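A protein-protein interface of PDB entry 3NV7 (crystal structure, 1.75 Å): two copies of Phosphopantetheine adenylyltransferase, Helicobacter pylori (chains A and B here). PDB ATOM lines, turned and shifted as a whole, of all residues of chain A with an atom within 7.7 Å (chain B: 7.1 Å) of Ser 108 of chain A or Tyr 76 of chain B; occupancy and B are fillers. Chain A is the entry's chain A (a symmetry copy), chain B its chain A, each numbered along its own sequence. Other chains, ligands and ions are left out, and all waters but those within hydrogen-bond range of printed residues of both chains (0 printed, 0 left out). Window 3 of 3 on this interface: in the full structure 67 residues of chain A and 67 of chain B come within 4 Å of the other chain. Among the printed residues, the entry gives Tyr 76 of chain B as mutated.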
ATOM      1  N   MET A 102      30.910   2.505 -24.987  1.00  0.00           N
ATOM      2  CA  MET A 102      31.773   3.328 -25.835  1.00  0.00           C
ATOM      3  C   MET A 102      31.921   2.744 -27.232  1.00  0.00           C
ATOM      4  O   MET A 102      31.916   3.486 -28.208  1.00  0.00           O
ATOM      5  CB  MET A 102      33.138   3.564 -25.188  1.00  0.00           C
ATOM      6  CG  MET A 102      33.101   4.575 -24.062  1.00  0.00           C
ATOM      7  SD  MET A 102      32.407   6.163 -24.581  1.00  0.00           S
ATOM      8  CE  MET A 102      30.764   6.122 -23.839  1.00  0.00           C
ATOM      9  N   GLY A 103      32.037   1.416 -27.315  1.00  0.00           N
ATOM     10  CA  GLY A 103      32.118   0.713 -28.599  1.00  0.00           C
ATOM     11  C   GLY A 103      30.915   1.017 -29.487  1.00  0.00           C
ATOM     12  O   GLY A 103      31.069   1.432 -30.650  1.00  0.00           O
ATOM     13  N   TYR A 104      29.717   0.824 -28.930  1.00  0.00           N
ATOM     14  CA  TYR A 104      28.471   1.084 -29.650  1.00  0.00           C
ATOM     15  C   TYR A 104      28.450   2.494 -30.238  1.00  0.00           C
ATOM     16  O   TYR A 104      28.228   2.671 -31.450  1.00  0.00           O
ATOM     17  CB  TYR A 104      27.254   0.828 -28.746  1.00  0.00           C
ATOM     18  CG  TYR A 104      27.123  -0.623 -28.328  1.00  0.00           C
ATOM     19  CD1 TYR A 104      27.440  -1.659 -29.224  1.00  0.00           C
ATOM     20  CD2 TYR A 104      26.671  -0.970 -27.051  1.00  0.00           C
ATOM     21  CE1 TYR A 104      27.325  -3.000 -28.853  1.00  0.00           C
ATOM     22  CE2 TYR A 104      26.550  -2.311 -26.672  1.00  0.00           C
ATOM     23  CZ  TYR A 104      26.881  -3.320 -27.580  1.00  0.00           C
ATOM     24  OH  TYR A 104      26.778  -4.651 -27.238  1.00  0.00           O
ATOM     25  N   ALA A 105      28.707   3.481 -29.378  1.00  0.00           N
ATOM     26  CA  ALA A 105      28.876   4.871 -29.793  1.00  0.00           C
ATOM     27  C   ALA A 105      29.881   5.017 -30.947  1.00  0.00           C
ATOM     28  O   ALA A 105      29.585   5.666 -31.959  1.00  0.00           O
ATOM     29  CB  ALA A 105      29.304   5.720 -28.606  1.00  0.00           C
ATOM     30  N   ASN A 106      31.043   4.374 -30.801  1.00  0.00           N
ATOM     31  CA  ASN A 106      32.186   4.574 -31.700  1.00  0.00           C
ATOM     32  C   ASN A 106      32.045   4.099 -33.155  1.00  0.00           C
ATOM     33  O   ASN A 106      33.052   3.972 -33.863  1.00  0.00           O
ATOM     34  CB  ASN A 106      33.488   4.041 -31.067  1.00  0.00           C
ATOM     35  CG  ASN A 106      34.139   5.046 -30.104  1.00  0.00           C
ATOM     36  OD1 ASN A 106      35.102   4.723 -29.409  1.00  0.00           O
ATOM     37  ND2 ASN A 106      33.611   6.261 -30.064  1.00  0.00           N
ATOM     38  N   LYS A 107      30.809   3.842 -33.596  1.00  0.00           N
ATOM     39  CA  LYS A 107      30.542   3.541 -35.014  1.00  0.00           C
ATOM     40  C   LYS A 107      29.143   3.957 -35.520  1.00  0.00           C
ATOM     41  O   LYS A 107      28.971   4.258 -36.714  1.00  0.00           O
ATOM     42  CB  LYS A 107      30.842   2.069 -35.341  1.00  0.00           C
ATOM     43  CG  LYS A 107      31.275   1.859 -36.796  1.00  0.00           C
ATOM     44  CD  LYS A 107      32.386   0.815 -36.925  1.00  0.00           C
ATOM     45  CE  LYS A 107      33.767   1.421 -36.664  1.00  0.00           C
ATOM     46  NZ  LYS A 107      34.851   0.399 -36.730  1.00  0.00           N
ATOM     47  N   SER A 108      28.158   3.988 -34.619  1.00  0.00           N
ATOM     48  CA  SER A 108      26.779   4.344 -34.986  1.00  0.00           C
ATOM     49  C   SER A 108      26.320   5.665 -34.358  1.00  0.00           C
ATOM     50  O   SER A 108      25.470   6.377 -34.924  1.00  0.00           O
ATOM     51  CB  SER A 108      25.810   3.215 -34.617  1.00  0.00           C
ATOM     52  OG  SER A 108      25.700   3.075 -33.211  1.00  0.00           O
ATOM     53  N   LEU A 109      26.875   5.975 -33.185  1.00  0.00           N
ATOM     54  CA  LEU A 109      26.609   7.249 -32.511  1.00  0.00           C
ATOM     55  C   LEU A 109      27.705   8.259 -32.860  1.00  0.00           C
ATOM     56  O   LEU A 109      28.142   8.314 -34.015  1.00  0.00           O
ATOM     57  CB  LEU A 109      26.466   7.051 -30.993  1.00  0.00           C
ATOM     58  CG  LEU A 109      25.115   6.567 -30.445  1.00  0.00           C
ATOM     59  CD1 LEU A 109      24.608   5.302 -31.127  1.00  0.00           C
ATOM     60  CD2 LEU A 109      25.198   6.363 -28.938  1.00  0.00           C
ATOM     61  N   ASN A 110      28.132   9.050 -31.873  1.00  0.00           N
ATOM     62  CA  ASN A 110      29.200  10.051 -32.043  1.00  0.00           C
ATOM     63  C   ASN A 110      30.419   9.600 -32.898  1.00  0.00           C
ATOM     64  O   ASN A 110      30.609  10.098 -34.019  1.00  0.00           O
ATOM     65  CB  ASN A 110      29.666  10.529 -30.664  1.00  0.00           C
ATOM     66  CG  ASN A 110      30.463  11.821 -30.714  1.00  0.00           C
ATOM     67  OD1 ASN A 110      31.019  12.235 -29.703  1.00  0.00           O
ATOM     68  ND2 ASN A 110      30.516  12.471 -31.883  1.00  0.00           N
ATOM     69  N   HIS A 111      31.229   8.677 -32.353  1.00  0.00           N
ATOM     70  CA  HIS A 111      32.405   8.082 -33.033  1.00  0.00           C
ATOM     71  C   HIS A 111      33.713   8.378 -32.310  1.00  0.00           C
ATOM     72  O   HIS A 111      33.759   9.260 -31.447  1.00  0.00           O
ATOM     73  CB  HIS A 111      32.529   8.529 -34.495  1.00  0.00           C
ATOM     74  CG  HIS A 111      31.796   7.650 -35.455  1.00  0.00           C
ATOM     75  ND1 HIS A 111      32.432   6.703 -36.229  1.00  0.00           N
ATOM     76  CD2 HIS A 111      30.481   7.569 -35.766  1.00  0.00           C
ATOM     77  CE1 HIS A 111      31.540   6.083 -36.981  1.00  0.00           C
ATOM     78  NE2 HIS A 111      30.348   6.590 -36.719  1.00  0.00           N
ATOM     79  N   LEU A 113      35.663   8.380 -29.927  1.00  0.00           N
ATOM     80  CA  LEU A 113      35.885   9.004 -28.617  1.00  0.00           C
ATOM     81  C   LEU A 113      36.977   8.277 -27.863  1.00  0.00           C
ATOM     82  O   LEU A 113      36.902   7.062 -27.693  1.00  0.00           O
ATOM     83  CB  LEU A 113      34.612   8.984 -27.771  1.00  0.00           C
ATOM     84  CG  LEU A 113      33.406   9.714 -28.340  1.00  0.00           C
ATOM     85  CD1 LEU A 113      32.206   9.491 -27.417  1.00  0.00           C
ATOM     86  CD2 LEU A 113      33.725  11.197 -28.532  1.00  0.00           C
ATOM     87  N   GLY B  72      21.110  11.320 -20.564  1.00  0.00           N
ATOM     88  CA  GLY B  72      21.739  10.153 -21.162  1.00  0.00           C
ATOM     89  C   GLY B  72      22.269  10.516 -22.526  1.00  0.00           C
ATOM     90  O   GLY B  72      22.297  11.706 -22.882  1.00  0.00           O
ATOM     91  N   LEU B  73      22.682   9.499 -23.285  1.00  0.00           N
ATOM     92  CA  LEU B  73      23.317   9.692 -24.598  1.00  0.00           C
ATOM     93  C   LEU B  73      24.624  10.501 -24.496  1.00  0.00           C
ATOM     94  O   LEU B  73      24.831  11.542 -25.170  1.00  0.00           O
ATOM     95  CB  LEU B  73      22.336  10.284 -25.620  1.00  0.00           C
ATOM     96  CG  LEU B  73      21.016   9.524 -25.839  1.00  0.00           C
ATOM     97  CD1 LEU B  73      20.023  10.301 -26.698  1.00  0.00           C
ATOM     98  CD2 LEU B  73      21.224   8.121 -26.435  1.00  0.00           C
ATOM     99  N   LEU B  74      25.523   9.982 -23.680  1.00  0.00           N
ATOM    100  CA  LEU B  74      26.830  10.582 -23.468  1.00  0.00           C
ATOM    101  C   LEU B  74      27.587  10.884 -24.769  1.00  0.00           C
ATOM    102  O   LEU B  74      28.188  11.967 -24.906  1.00  0.00           O
ATOM    103  CB  LEU B  74      27.665   9.668 -22.540  1.00  0.00           C
ATOM    104  CG  LEU B  74      29.103  10.167 -22.288  1.00  0.00           C
ATOM    105  CD1 LEU B  74      29.174  11.598 -21.641  1.00  0.00           C
ATOM    106  CD2 LEU B  74      29.871   9.135 -21.449  1.00  0.00           C
ATOM    107  N   ALA B  75      27.545   9.963 -25.738  1.00  0.00           N
ATOM    108  CA  ALA B  75      28.294  10.193 -26.974  1.00  0.00           C
ATOM    109  C   ALA B  75      27.715  11.396 -27.733  1.00  0.00           C
ATOM    110  O   ALA B  75      28.458  12.176 -28.339  1.00  0.00           O
ATOM    111  CB  ALA B  75      28.294   8.973 -27.853  1.00  0.00           C
ATOM    112  N   TYR B  76      26.395  11.560 -27.692  1.00  0.00           N
ATOM    113  CA  TYR B  76      25.784  12.748 -28.270  1.00  0.00           C
ATOM    114  C   TYR B  76      26.007  14.052 -27.469  1.00  0.00           C
ATOM    115  O   TYR B  76      26.114  15.155 -28.050  1.00  0.00           O
ATOM    116  CB  TYR B  76      24.315  12.483 -28.598  1.00  0.00           C
ATOM    117  CG  TYR B  76      24.185  11.585 -29.802  1.00  0.00           C
ATOM    118  CD1 TYR B  76      24.735  11.958 -31.033  1.00  0.00           C
ATOM    119  CD2 TYR B  76      23.492  10.397 -29.734  1.00  0.00           C
ATOM    120  CE1 TYR B  76      24.613  11.143 -32.175  1.00  0.00           C
ATOM    121  CE2 TYR B  76      23.359   9.568 -30.876  1.00  0.00           C
ATOM    122  CZ  TYR B  76      23.922   9.950 -32.076  1.00  0.00           C
ATOM    123  OH  TYR B  76      23.786   9.154 -33.190  1.00  0.00           O
ATOM    124  N   LEU B  77      26.162  13.919 -26.154  1.00  0.00           N
ATOM    125  CA  LEU B  77      26.555  15.046 -25.340  1.00  0.00           C
ATOM    126  C   LEU B  77      27.967  15.468 -25.763  1.00  0.00           C
ATOM    127  O   LEU B  77      28.213  16.668 -25.974  1.00  0.00           O
ATOM    128  CB  LEU B  77      26.504  14.676 -23.845  1.00  0.00           C
ATOM    129  CG  LEU B  77      26.840  15.814 -22.873  1.00  0.00           C
ATOM    130  CD1 LEU B  77      25.648  16.761 -22.727  1.00  0.00           C
ATOM    131  CD2 LEU B  77      27.228  15.224 -21.521  1.00  0.00           C
ATOM    132  N   ALA B  78      28.864  14.477 -25.936  1.00  0.00           N
ATOM    133  CA  ALA B  78      30.222  14.753 -26.446  1.00  0.00           C
ATOM    134  C   ALA B  78      30.166  15.492 -27.789  1.00  0.00           C
ATOM    135  O   ALA B  78      30.879  16.491 -27.979  1.00  0.00           O
ATOM    136  CB  ALA B  78      31.057  13.484 -26.558  1.00  0.00           C
ATOM    137  N   LYS B  79      29.307  15.021 -28.703  1.00  0.00           N
ATOM    138  CA  LYS B  79      29.125  15.669 -30.015  1.00  0.00           C
ATOM    139  C   LYS B  79      28.745  17.145 -29.863  1.00  0.00           C
ATOM    140  O   LYS B  79      29.301  18.028 -30.553  1.00  0.00           O
ATOM    141  CB  LYS B  79      28.054  14.925 -30.829  1.00  0.00           C
ATOM    142  CG  LYS B  79      28.106  15.244 -32.335  1.00  0.00           C
ATOM    143  CD  LYS B  79      26.921  14.630 -33.087  1.00  0.00           C
ATOM    144  CE  LYS B  79      26.734  15.310 -34.435  1.00  0.00           C
ATOM    145  NZ  LYS B  79      27.906  15.112 -35.312  1.00  0.00           N
ATOM    146  N   GLU B  80      27.789  17.425 -28.979  1.00  0.00           N
ATOM    147  CA  GLU B  80      27.339  18.814 -28.751  1.00  0.00           C
ATOM    148  C   GLU B  80      28.502  19.731 -28.332  1.00  0.00           C
ATOM    149  O   GLU B  80      28.551  20.900 -28.740  1.00  0.00           O
ATOM    150  CB  GLU B  80      26.199  18.857 -27.705  1.00  0.00           C
ATOM    151  CG  GLU B  80      25.796  20.271 -27.197  1.00  0.00           C
ATOM    152  CD  GLU B  80      25.317  21.203 -28.294  1.00  0.00           C
ATOM    153  OE1 GLU B  80      24.844  20.731 -29.340  1.00  0.00           O
ATOM    154  OE2 GLU B  80      25.399  22.424 -28.098  1.00  0.00           O
ATOM    155  N   TYR B  81      29.457  19.187 -27.564  1.00  0.00           N
ATOM    156  CA  TYR B  81      30.594  19.965 -27.084  1.00  0.00           C
ATOM    157  C   TYR B  81      31.810  19.953 -28.031  1.00  0.00           C
ATOM    158  O   TYR B  81      32.833  20.578 -27.722  1.00  0.00           O
ATOM    159  CB  TYR B  81      30.968  19.532 -25.642  1.00  0.00           C
ATOM    160  CG  TYR B  81      29.994  20.100 -24.636  1.00  0.00           C
ATOM    161  CD1 TYR B  81      30.222  21.342 -24.035  1.00  0.00           C
ATOM    162  CD2 TYR B  81      28.831  19.425 -24.312  1.00  0.00           C
ATOM    163  CE1 TYR B  81      29.306  21.893 -23.142  1.00  0.00           C
ATOM    164  CE2 TYR B  81      27.906  19.963 -23.419  1.00  0.00           C
ATOM    165  CZ  TYR B  81      28.139  21.199 -22.845  1.00  0.00           C
ATOM    166  OH  TYR B  81      27.210  21.729 -21.951  1.00  0.00           O
ATOM    167  N   HIS B  82      31.680  19.295 -29.190  1.00  0.00           N
ATOM    168  CA  HIS B  82      32.823  19.046 -30.090  1.00  0.00           C
ATOM    169  C   HIS B  82      33.945  18.365 -29.318  1.00  0.00           C
ATOM    170  O   HIS B  82      35.120  18.719 -29.467  1.00  0.00           O
ATOM    171  CB  HIS B  82      33.345  20.359 -30.708  1.00  0.00           C
ATOM    172  CG  HIS B  82      32.283  21.159 -31.391  1.00  0.00           C
ATOM    173  ND1 HIS B  82      31.563  20.673 -32.460  1.00  0.00           N
ATOM    174  CD2 HIS B  82      31.799  22.402 -31.144  1.00  0.00           C
ATOM    175  CE1 HIS B  82      30.683  21.580 -32.849  1.00  0.00           C
ATOM    176  NE2 HIS B  82      30.806  22.640 -32.068  1.00  0.00           N
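The backbone carbonyl oxygen (O) of Ala 75 of chain B sits close to the side-chain amide oxygen (OD1) of Asn 110 of chain A (2.9 Å).
N of Lys 79 of chain B sits at hydrogen-bond distance from OD1 of Asn 110 of chain A (3.4 Å).
The backbone carbonyl oxygen (O) of Tyr 104 of chain A is in hydrogen-bond range of the side-chain hydroxyl (OG) of Ser 108 of chain A (3.1 Å).
N of His 111 of chain A is in hydrogen-bond range of O of Ala 105 of chain A, 3.5 Å away.
ND2 of Asn 106 of chain A sits close to N of Leu 113 of chain A (3.0 Å).
Met 102 of chain A touches Leu 74 of chain B (CE to CD2, 3.9 Å).
Ala 75 of chain B touches Ala 105 of chain A (CB to CB, 3.5 Å).
Tyr 76 of chain B touches Ser 108 of chain A (OH to O, 3.7 Å).
Tyr 76 of chain B touches Leu 109 of chain A.
OD1 of Asn 110 of chain A touches CB of Ala 78 of chain B (3.4 Å).
CB of Ala 75 of chain B touches CD1 of Leu 113 of chain A (3.97 Å).
Ser 108 of chain A touches just one residue of chain B: Tyr 76.
Of chain A, only Ser 108 and Leu 109 come within 4 Å of Tyr 76 of chain B.
Of the printed residues of chain A, Ala 78 of chain B touches Asn 110.
Of the printed residues of chain A, Lys 79 of chain B touches Asn 110.
His 82 of chain B touches none of the printed residues of chain A.
Leu 77 of chain B touches none of the printed residues of chain A.
The nearest printed residue of chain B that does not touch Ser 108 of chain A is Ala 75 of chain B (7.6 Å).
The nearest printed residue of chain A that does not touch Leu 74 of chain B is Leu 113 of chain A (5.3 Å).
Printed residues of chain A that touch a printed residue of chain B: Met 102, Ala 105, Ser 108, Leu 109, Asn 110 and Leu 113.
Of the 11 printed residues of chain B, 5 touch a printed residue of chain A.
Among the printed residues, no Asp or Glu carboxylate lies within 4 Å of a Lys or Arg side-chain nitrogen of the other chain.
No position is printed for both chains.
Of the 8 pairs that touch across the chains among the printed residues, none has its exchanged pair printed and touching as well.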
